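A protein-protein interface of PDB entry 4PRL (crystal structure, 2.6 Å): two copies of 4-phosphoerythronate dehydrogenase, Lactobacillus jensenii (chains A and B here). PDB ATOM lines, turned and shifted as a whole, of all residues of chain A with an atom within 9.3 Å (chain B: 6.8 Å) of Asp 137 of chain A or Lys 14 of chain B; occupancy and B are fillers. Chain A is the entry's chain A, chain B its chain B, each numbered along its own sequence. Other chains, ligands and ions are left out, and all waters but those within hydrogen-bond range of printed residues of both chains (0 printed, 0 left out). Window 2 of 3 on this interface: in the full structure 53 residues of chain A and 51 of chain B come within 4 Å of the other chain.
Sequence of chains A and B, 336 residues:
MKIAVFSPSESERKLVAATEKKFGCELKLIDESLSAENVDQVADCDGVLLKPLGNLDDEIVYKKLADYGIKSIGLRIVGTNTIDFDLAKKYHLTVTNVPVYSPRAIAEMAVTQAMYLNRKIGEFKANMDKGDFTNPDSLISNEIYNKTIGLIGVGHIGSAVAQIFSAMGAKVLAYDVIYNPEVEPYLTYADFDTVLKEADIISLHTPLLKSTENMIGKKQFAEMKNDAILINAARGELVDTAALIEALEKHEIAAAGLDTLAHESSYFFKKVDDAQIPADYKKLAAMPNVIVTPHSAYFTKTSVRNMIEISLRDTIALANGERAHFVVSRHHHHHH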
ATOM      1  N   LYS A 120     -25.378  -8.405 -19.123  1.00  0.00           N
ATOM      2  CA  LYS A 120     -25.770  -7.310 -19.989  1.00  0.00           C
ATOM      3  C   LYS A 120     -24.981  -7.295 -21.282  1.00  0.00           C
ATOM      4  O   LYS A 120     -24.649  -6.238 -21.808  1.00  0.00           O
ATOM      5  CB  LYS A 120     -25.595  -5.982 -19.267  1.00  0.00           C
ATOM      6  CG  LYS A 120     -26.432  -5.871 -18.012  1.00  0.00           C
ATOM      7  CD  LYS A 120     -26.145  -4.582 -17.270  1.00  0.00           C
ATOM      8  CE  LYS A 120     -27.081  -4.436 -16.092  1.00  0.00           C
ATOM      9  NZ  LYS A 120     -26.481  -3.552 -15.070  1.00  0.00           N
ATOM     10  N   GLU A 123     -26.496  -5.280 -24.181  1.00  0.00           N
ATOM     11  CA  GLU A 123     -26.464  -3.835 -23.984  1.00  0.00           C
ATOM     12  C   GLU A 123     -25.061  -3.331 -24.292  1.00  0.00           C
ATOM     13  O   GLU A 123     -24.899  -2.297 -24.941  1.00  0.00           O
ATOM     14  CB  GLU A 123     -26.903  -3.447 -22.572  1.00  0.00           C
ATOM     15  CG  GLU A 123     -28.327  -3.865 -22.208  1.00  0.00           C
ATOM     16  CD  GLU A 123     -28.664  -3.577 -20.746  1.00  0.00           C
ATOM     17  OE1 GLU A 123     -28.742  -2.387 -20.395  1.00  0.00           O
ATOM     18  OE2 GLU A 123     -28.851  -4.521 -19.938  1.00  0.00           O
ATOM     19  N   PHE A 124     -24.043  -4.069 -23.860  1.00  0.00           N
ATOM     20  CA  PHE A 124     -22.679  -3.788 -24.314  1.00  0.00           C
ATOM     21  C   PHE A 124     -22.559  -3.804 -25.821  1.00  0.00           C
ATOM     22  O   PHE A 124     -21.868  -2.964 -26.380  1.00  0.00           O
ATOM     23  CB  PHE A 124     -21.680  -4.816 -23.811  1.00  0.00           C
ATOM     24  CG  PHE A 124     -21.192  -4.569 -22.422  1.00  0.00           C
ATOM     25  CD1 PHE A 124     -20.293  -3.553 -22.172  1.00  0.00           C
ATOM     26  CD2 PHE A 124     -21.603  -5.388 -21.374  1.00  0.00           C
ATOM     27  CE1 PHE A 124     -19.829  -3.326 -20.909  1.00  0.00           C
ATOM     28  CE2 PHE A 124     -21.148  -5.162 -20.117  1.00  0.00           C
ATOM     29  CZ  PHE A 124     -20.254  -4.133 -19.882  1.00  0.00           C
ATOM     30  N   ASN A 127     -24.056  -0.737 -27.412  1.00  0.00           N
ATOM     31  CA  ASN A 127     -23.079   0.338 -27.297  1.00  0.00           C
ATOM     32  C   ASN A 127     -21.928   0.266 -28.289  1.00  0.00           C
ATOM     33  O   ASN A 127     -21.619   1.245 -28.972  1.00  0.00           O
ATOM     34  CB  ASN A 127     -22.478   0.363 -25.901  1.00  0.00           C
ATOM     35  CG  ASN A 127     -23.097   1.422 -25.026  1.00  0.00           C
ATOM     36  OD1 ASN A 127     -24.205   1.895 -25.283  1.00  0.00           O
ATOM     37  ND2 ASN A 127     -22.379   1.802 -23.986  1.00  0.00           N
ATOM     38  N   ASP A 132     -19.172   2.967 -28.708  1.00  0.00           N
ATOM     39  CA  ASP A 132     -18.867   3.093 -27.283  1.00  0.00           C
ATOM     40  C   ASP A 132     -18.328   1.786 -26.704  1.00  0.00           C
ATOM     41  O   ASP A 132     -19.077   0.808 -26.580  1.00  0.00           O
ATOM     42  CB  ASP A 132     -20.132   3.526 -26.541  1.00  0.00           C
ATOM     43  CG  ASP A 132     -19.867   3.923 -25.107  1.00  0.00           C
ATOM     44  OD1 ASP A 132     -18.903   3.400 -24.492  1.00  0.00           O
ATOM     45  OD2 ASP A 132     -20.639   4.760 -24.592  1.00  0.00           O
ATOM     46  N   THR A 134     -16.652   1.645 -23.610  1.00  0.00           N
ATOM     47  CA  THR A 134     -16.388   1.903 -22.210  1.00  0.00           C
ATOM     48  C   THR A 134     -17.129   0.913 -21.288  1.00  0.00           C
ATOM     49  O   THR A 134     -17.818  -0.008 -21.741  1.00  0.00           O
ATOM     50  CB  THR A 134     -16.800   3.353 -21.839  1.00  0.00           C
ATOM     51  OG1 THR A 134     -18.203   3.533 -22.081  1.00  0.00           O
ATOM     52  CG2 THR A 134     -16.009   4.375 -22.661  1.00  0.00           C
ATOM     53  N   ASN A 135     -16.954   1.130 -19.988  1.00  0.00           N
ATOM     54  CA  ASN A 135     -17.616   0.383 -18.938  1.00  0.00           C
ATOM     55  C   ASN A 135     -18.418   1.358 -18.061  1.00  0.00           C
ATOM     56  O   ASN A 135     -18.063   1.608 -16.913  1.00  0.00           O
ATOM     57  CB  ASN A 135     -16.573  -0.332 -18.064  1.00  0.00           C
ATOM     58  CG  ASN A 135     -15.778  -1.394 -18.810  1.00  0.00           C
ATOM     59  OD1 ASN A 135     -14.788  -1.892 -18.280  1.00  0.00           O
ATOM     60  ND2 ASN A 135     -16.201  -1.749 -20.030  1.00  0.00           N
ATOM     61  N   PRO A 136     -19.503   1.913 -18.600  1.00  0.00           N
ATOM     62  CA  PRO A 136     -20.287   2.811 -17.788  1.00  0.00           C
ATOM     63  C   PRO A 136     -20.945   2.044 -16.656  1.00  0.00           C
ATOM     64  O   PRO A 136     -21.109   0.852 -16.761  1.00  0.00           O
ATOM     65  CB  PRO A 136     -21.336   3.350 -18.768  1.00  0.00           C
ATOM     66  CG  PRO A 136     -21.498   2.281 -19.781  1.00  0.00           C
ATOM     67  CD  PRO A 136     -20.167   1.582 -19.876  1.00  0.00           C
ATOM     68  N   ASP A 137     -21.331   2.737 -15.591  1.00  0.00           N
ATOM     69  CA  ASP A 137     -21.889   2.104 -14.402  1.00  0.00           C
ATOM     70  C   ASP A 137     -23.280   1.525 -14.640  1.00  0.00           C
ATOM     71  O   ASP A 137     -23.748   0.660 -13.900  1.00  0.00           O
ATOM     72  CB  ASP A 137     -21.968   3.118 -13.292  1.00  0.00           C
ATOM     73  CG  ASP A 137     -22.434   2.519 -12.021  1.00  0.00           C
ATOM     74  OD1 ASP A 137     -21.654   1.744 -11.437  1.00  0.00           O
ATOM     75  OD2 ASP A 137     -23.565   2.823 -11.604  1.00  0.00           O
ATOM     76  N   SER A 138     -23.932   1.999 -15.688  1.00  0.00           N
ATOM     77  CA  SER A 138     -25.240   1.516 -16.034  1.00  0.00           C
ATOM     78  C   SER A 138     -25.175   0.111 -16.602  1.00  0.00           C
ATOM     79  O   SER A 138     -26.217  -0.507 -16.812  1.00  0.00           O
ATOM     80  CB  SER A 138     -25.859   2.446 -17.067  1.00  0.00           C
ATOM     81  OG  SER A 138     -25.078   2.430 -18.236  1.00  0.00           O
ATOM     82  N   LEU A 139     -23.966  -0.374 -16.893  1.00  0.00           N
ATOM     83  CA  LEU A 139     -23.757  -1.762 -17.351  1.00  0.00           C
ATOM     84  C   LEU A 139     -22.932  -2.595 -16.383  1.00  0.00           C
ATOM     85  O   LEU A 139     -22.353  -3.603 -16.763  1.00  0.00           O
ATOM     86  CB  LEU A 139     -23.048  -1.765 -18.698  1.00  0.00           C
ATOM     87  CG  LEU A 139     -23.780  -1.002 -19.792  1.00  0.00           C
ATOM     88  CD1 LEU A 139     -22.995  -1.130 -21.093  1.00  0.00           C
ATOM     89  CD2 LEU A 139     -25.197  -1.533 -19.931  1.00  0.00           C
ATOM     90  N   ILE A 140     -22.858  -2.177 -15.133  1.00  0.00           N
ATOM     91  CA  ILE A 140     -22.098  -2.940 -14.153  1.00  0.00           C
ATOM     92  C   ILE A 140     -22.918  -4.179 -13.828  1.00  0.00           C
ATOM     93  O   ILE A 140     -24.144  -4.137 -13.857  1.00  0.00           O
ATOM     94  CB  ILE A 140     -21.803  -2.102 -12.896  1.00  0.00           C
ATOM     95  CG1 ILE A 140     -20.663  -2.705 -12.104  1.00  0.00           C
ATOM     96  CG2 ILE A 140     -23.037  -1.941 -12.020  1.00  0.00           C
ATOM     97  CD1 ILE A 140     -20.348  -1.895 -10.850  1.00  0.00           C
ATOM     98  N   SER A 141     -22.253  -5.292 -13.554  1.00  0.00           N
ATOM     99  CA  SER A 141     -22.974  -6.537 -13.290  1.00  0.00           C
ATOM    100  C   SER A 141     -22.728  -6.996 -11.864  1.00  0.00           C
ATOM    101  O   SER A 141     -22.359  -6.206 -10.985  1.00  0.00           O
ATOM    102  CB  SER A 141     -22.578  -7.626 -14.300  1.00  0.00           C
ATOM    103  OG  SER A 141     -23.480  -8.725 -14.258  1.00  0.00           O
ATOM    104  N   ASN A 142     -22.981  -8.276 -11.629  1.00  0.00           N
ATOM    105  CA  ASN A 142     -22.759  -8.863 -10.320  1.00  0.00           C
ATOM    106  C   ASN A 142     -22.589 -10.392 -10.413  1.00  0.00           C
ATOM    107  O   ASN A 142     -23.015 -11.042 -11.377  1.00  0.00           O
ATOM    108  CB  ASN A 142     -23.899  -8.484  -9.354  1.00  0.00           C
ATOM    109  CG  ASN A 142     -23.450  -8.407  -7.888  1.00  0.00           C
ATOM    110  OD1 ASN A 142     -22.263  -8.500  -7.566  1.00  0.00           O
ATOM    111  ND2 ASN A 142     -24.409  -8.232  -6.997  1.00  0.00           N
ATOM    112  N   SER B   9     -13.647   6.012 -11.552  1.00  0.00           N
ATOM    113  CA  SER B   9     -14.707   5.621 -12.452  1.00  0.00           C
ATOM    114  C   SER B   9     -16.021   6.114 -11.905  1.00  0.00           C
ATOM    115  O   SER B   9     -16.187   6.301 -10.699  1.00  0.00           O
ATOM    116  CB  SER B   9     -14.757   4.092 -12.629  1.00  0.00           C
ATOM    117  OG  SER B   9     -15.255   3.398 -11.483  1.00  0.00           O
ATOM    118  N   GLU B  10     -16.954   6.331 -12.814  1.00  0.00           N
ATOM    119  CA  GLU B  10     -18.376   6.437 -12.499  1.00  0.00           C
ATOM    120  C   GLU B  10     -18.785   5.422 -11.407  1.00  0.00           C
ATOM    121  O   GLU B  10     -19.478   5.783 -10.445  1.00  0.00           O
ATOM    122  CB  GLU B  10     -19.144   6.191 -13.794  1.00  0.00           C
ATOM    123  CG  GLU B  10     -20.540   6.750 -13.890  1.00  0.00           C
ATOM    124  CD  GLU B  10     -21.034   6.703 -15.332  1.00  0.00           C
ATOM    125  OE1 GLU B  10     -21.525   5.645 -15.773  1.00  0.00           O
ATOM    126  OE2 GLU B  10     -20.910   7.719 -16.047  1.00  0.00           O
ATOM    127  N   SER B  11     -18.344   4.163 -11.529  1.00  0.00           N
ATOM    128  CA  SER B  11     -18.713   3.123 -10.538  1.00  0.00           C
ATOM    129  C   SER B  11     -18.038   3.307  -9.191  1.00  0.00           C
ATOM    130  O   SER B  11     -18.633   3.041  -8.158  1.00  0.00           O
ATOM    131  CB  SER B  11     -18.415   1.722 -11.058  1.00  0.00           C
ATOM    132  OG  SER B  11     -19.322   1.383 -12.092  1.00  0.00           O
ATOM    133  N   GLU B  12     -16.793   3.756  -9.201  1.00  0.00           N
ATOM    134  CA  GLU B  12     -16.100   4.046  -7.955  1.00  0.00           C
ATOM    135  C   GLU B  12     -16.742   5.238  -7.247  1.00  0.00           C
ATOM    136  O   GLU B  12     -16.946   5.201  -6.035  1.00  0.00           O
ATOM    137  CB  GLU B  12     -14.624   4.276  -8.201  1.00  0.00           C
ATOM    138  CG  GLU B  12     -13.937   3.060  -8.788  1.00  0.00           C
ATOM    139  CD  GLU B  12     -12.489   3.313  -9.149  1.00  0.00           C
ATOM    140  OE1 GLU B  12     -12.221   4.291  -9.876  1.00  0.00           O
ATOM    141  OE2 GLU B  12     -11.624   2.507  -8.742  1.00  0.00           O
ATOM    142  N   ARG B  13     -17.139   6.266  -7.983  1.00  0.00           N
ATOM    143  CA  ARG B  13     -17.868   7.366  -7.333  1.00  0.00           C
ATOM    144  C   ARG B  13     -19.062   6.908  -6.472  1.00  0.00           C
ATOM    145  O   ARG B  13     -19.306   7.452  -5.402  1.00  0.00           O
ATOM    146  CB  ARG B  13     -18.325   8.407  -8.358  1.00  0.00           C
ATOM    147  CG  ARG B  13     -17.178   9.185  -8.985  1.00  0.00           C
ATOM    148  CD  ARG B  13     -17.614  10.039 -10.164  1.00  0.00           C
ATOM    149  NE  ARG B  13     -16.475  10.425 -11.016  1.00  0.00           N
ATOM    150  CZ  ARG B  13     -15.692  11.476 -10.790  1.00  0.00           C
ATOM    151  NH1 ARG B  13     -15.923  12.248  -9.732  1.00  0.00           N
ATOM    152  NH2 ARG B  13     -14.684  11.756 -11.621  1.00  0.00           N
ATOM    153  N   LYS B  14     -19.793   5.897  -6.914  1.00  0.00           N
ATOM    154  CA  LYS B  14     -20.970   5.464  -6.162  1.00  0.00           C
ATOM    155  C   LYS B  14     -20.604   4.842  -4.816  1.00  0.00           C
ATOM    156  O   LYS B  14     -21.455   4.734  -3.953  1.00  0.00           O
ATOM    157  CB  LYS B  14     -21.814   4.447  -6.947  1.00  0.00           C
ATOM    158  CG  LYS B  14     -22.097   4.767  -8.408  1.00  0.00           C
ATOM    159  CD  LYS B  14     -22.541   6.199  -8.663  1.00  0.00           C
ATOM    160  CE  LYS B  14     -23.475   6.253  -9.867  1.00  0.00           C
ATOM    161  NZ  LYS B  14     -23.806   7.643 -10.277  1.00  0.00           N
ATOM    162  N   LEU B  15     -19.352   4.429  -4.649  1.00  0.00           N
ATOM    163  CA  LEU B  15     -18.898   3.727  -3.451  1.00  0.00           C
ATOM    164  C   LEU B  15     -18.354   4.627  -2.393  1.00  0.00           C
ATOM    165  O   LEU B  15     -18.116   4.165  -1.290  1.00  0.00           O
ATOM    166  CB  LEU B  15     -17.735   2.796  -3.799  1.00  0.00           C
ATOM    167  CG  LEU B  15     -18.095   1.621  -4.684  1.00  0.00           C
ATOM    168  CD1 LEU B  15     -16.834   0.893  -5.120  1.00  0.00           C
ATOM    169  CD2 LEU B  15     -19.071   0.701  -3.942  1.00  0.00           C
ATOM    170  N   VAL B  16     -18.098   5.886  -2.724  1.00  0.00           N
ATOM    171  CA  VAL B  16     -17.241   6.706  -1.870  1.00  0.00           C
ATOM    172  C   VAL B  16     -17.744   6.795  -0.423  1.00  0.00           C
ATOM    173  O   VAL B  16     -16.985   6.570   0.501  1.00  0.00           O
ATOM    174  CB  VAL B  16     -17.010   8.123  -2.439  1.00  0.00           C
ATOM    175  CG1 VAL B  16     -16.165   8.949  -1.475  1.00  0.00           C
ATOM    176  CG2 VAL B  16     -16.316   8.050  -3.791  1.00  0.00           C
ATOM    177  N   ALA B  17     -19.010   7.101  -0.218  1.00  0.00           N
ATOM    178  CA  ALA B  17     -19.492   7.334   1.146  1.00  0.00           C
ATOM    179  C   ALA B  17     -19.354   6.069   1.942  1.00  0.00           C
ATOM    180  O   ALA B  17     -18.865   6.091   3.060  1.00  0.00           O
ATOM    181  CB  ALA B  17     -20.944   7.829   1.161  1.00  0.00           C
ATOM    182  N   ALA B  18     -19.775   4.952   1.360  1.00  0.00           N
ATOM    183  CA  ALA B  18     -19.718   3.681   2.073  1.00  0.00           C
ATOM    184  C   ALA B  18     -18.290   3.442   2.539  1.00  0.00           C
ATOM    185  O   ALA B  18     -18.029   3.127   3.709  1.00  0.00           O
ATOM    186  CB  ALA B  18     -20.191   2.544   1.179  1.00  0.00           C
ATOM    187  N   LEU B  29     -11.532  12.793  -4.644  1.00  0.00           N
ATOM    188  CA  LEU B  29     -11.542  12.347  -6.030  1.00  0.00           C
ATOM    189  C   LEU B  29     -11.066  13.443  -6.972  1.00  0.00           C
ATOM    190  O   LEU B  29     -11.479  14.591  -6.840  1.00  0.00           O
ATOM    191  CB  LEU B  29     -12.947  11.924  -6.430  1.00  0.00           C
ATOM    192  CG  LEU B  29     -13.394  10.541  -5.978  1.00  0.00           C
ATOM    193  CD1 LEU B  29     -12.977  10.205  -4.562  1.00  0.00           C
ATOM    194  CD2 LEU B  29     -14.908  10.468  -6.103  1.00  0.00           C
ATOM    195  N   PHE B 299     -16.182  -6.599 -14.639  1.00  0.00           N
ATOM    196  CA  PHE B 299     -17.033  -5.464 -14.260  1.00  0.00           C
ATOM    197  C   PHE B 299     -18.283  -5.841 -13.457  1.00  0.00           C
ATOM    198  O   PHE B 299     -19.413  -5.897 -13.999  1.00  0.00           O
ATOM    199  CB  PHE B 299     -17.412  -4.685 -15.522  1.00  0.00           C
ATOM    200  CG  PHE B 299     -17.898  -3.269 -15.279  1.00  0.00           C
ATOM    201  CD1 PHE B 299     -17.388  -2.475 -14.253  1.00  0.00           C
ATOM    202  CD2 PHE B 299     -18.837  -2.711 -16.140  1.00  0.00           C
ATOM    203  CE1 PHE B 299     -17.842  -1.177 -14.071  1.00  0.00           C
ATOM    204  CE2 PHE B 299     -19.291  -1.426 -15.970  1.00  0.00           C
ATOM    205  CZ  PHE B 299     -18.788  -0.651 -14.939  1.00  0.00           C
ATOM    206  N   LYS B 301     -19.894  -5.229  -9.172  1.00  0.00           N
ATOM    207  CA  LYS B 301     -19.868  -4.415  -7.953  1.00  0.00           C
ATOM    208  C   LYS B 301     -18.723  -4.837  -7.020  1.00  0.00           C
ATOM    209  O   LYS B 301     -17.977  -4.010  -6.476  1.00  0.00           O
ATOM    210  CB  LYS B 301     -21.172  -4.576  -7.194  1.00  0.00           C
ATOM    211  CG  LYS B 301     -22.446  -4.390  -8.012  1.00  0.00           C
ATOM    212  CD  LYS B 301     -23.072  -3.013  -7.857  1.00  0.00           C
ATOM    213  CE  LYS B 301     -24.595  -3.111  -7.840  1.00  0.00           C
ATOM    214  NZ  LYS B 301     -25.251  -1.794  -7.579  1.00  0.00           N
ATOM    215  N   VAL B 304     -15.183  -3.864  -8.436  1.00  0.00           N
ATOM    216  CA  VAL B 304     -15.038  -2.429  -8.247  1.00  0.00           C
ATOM    217  C   VAL B 304     -14.828  -2.087  -6.773  1.00  0.00           C
ATOM    218  O   VAL B 304     -13.914  -1.360  -6.446  1.00  0.00           O
ATOM    219  CB  VAL B 304     -16.258  -1.705  -8.853  1.00  0.00           C
ATOM    220  CG1 VAL B 304     -16.327  -0.251  -8.419  1.00  0.00           C
ATOM    221  CG2 VAL B 304     -16.206  -1.819 -10.368  1.00  0.00           C
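The backbone carbonyl oxygen (O) of Phe 299 of chain B lies within hydrogen-bond range of the backbone NH (N) of Ser 141 of chain A (2.9 Å). The side-chain carboxylate of Glu 10 of chain B is in hydrogen-bond range of the backbone NH of Asp 137 of chain A (2.9 Å). OD1 of Asp 137 of chain A is in hydrogen-bond range of OG of Ser 11 of chain B, 2.4 Å away. N of Lys 301 of chain B is in hydrogen-bond range of O of Ser 141 of chain A (3.2 Å).
OG of Ser 9 of chain B lies close to N of Ser 11 of chain B, 3.2 Å away. The side-chain amino group of Lys 120 of chain A is in hydrogen-bond range of the backbone carbonyl oxygen of Ile 140 of chain A.
Asn 135 of chain A touches Phe 299 of chain B (O to CZ, 3.1 Å). Pro 136 of chain A touches Glu 10 of chain B. O of Pro 136 of chain A touches CE2 of Phe 299 of chain B, 3.0 Å away. Lys 14 of chain B touches Asp 137 of chain A (CE to OD2, 3.8 Å). Leu 139 of chain A touches Phe 299 of chain B. OG of Ser 11 of chain B touches CD1 of Ile 140 of chain A, at 3.7 Å. Phe 299 of chain B touches Ile 140 of chain A. Lys 301 of chain B touches Ile 140 of chain A (N to CD1, 3.8 Å).
Of the printed residues of chain B, Asn 135 of chain A touches Phe 299. Of the printed residues of chain B, Leu 139 of chain A touches Phe 299 (3.7 Å). Of the printed residues of chain A, Lys 14 of chain B touches Asp 137. Of the printed residues of chain A, Phe 299 of chain B touches Asn 135, Pro 136, Leu 139, Ile 140 and Ser 141. The nearest residue of chain B that does not touch Asp 137 of chain A is Phe 299 of chain B (4.2 Å).
Of the 14 printed residues of chain B, 5 touch a printed residue of chain A. Hydrophobic or aromatic side chains of chain B within 4 Å of the printed part of chain A: Phe 299. Of the 14 printed residues of chain A, 6 touch a printed residue of chain B. Among the printed residues, 12 pairs touch across the chains. Among the printed residues, no Asp or Glu carboxylate lies within 4 Å of a Lys or Arg side-chain nitrogen of the other chain.
No position is printed for both chains. Of the 12 pairs that touch across the chains among the printed residues, none has its exchanged pair printed and touching as well.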
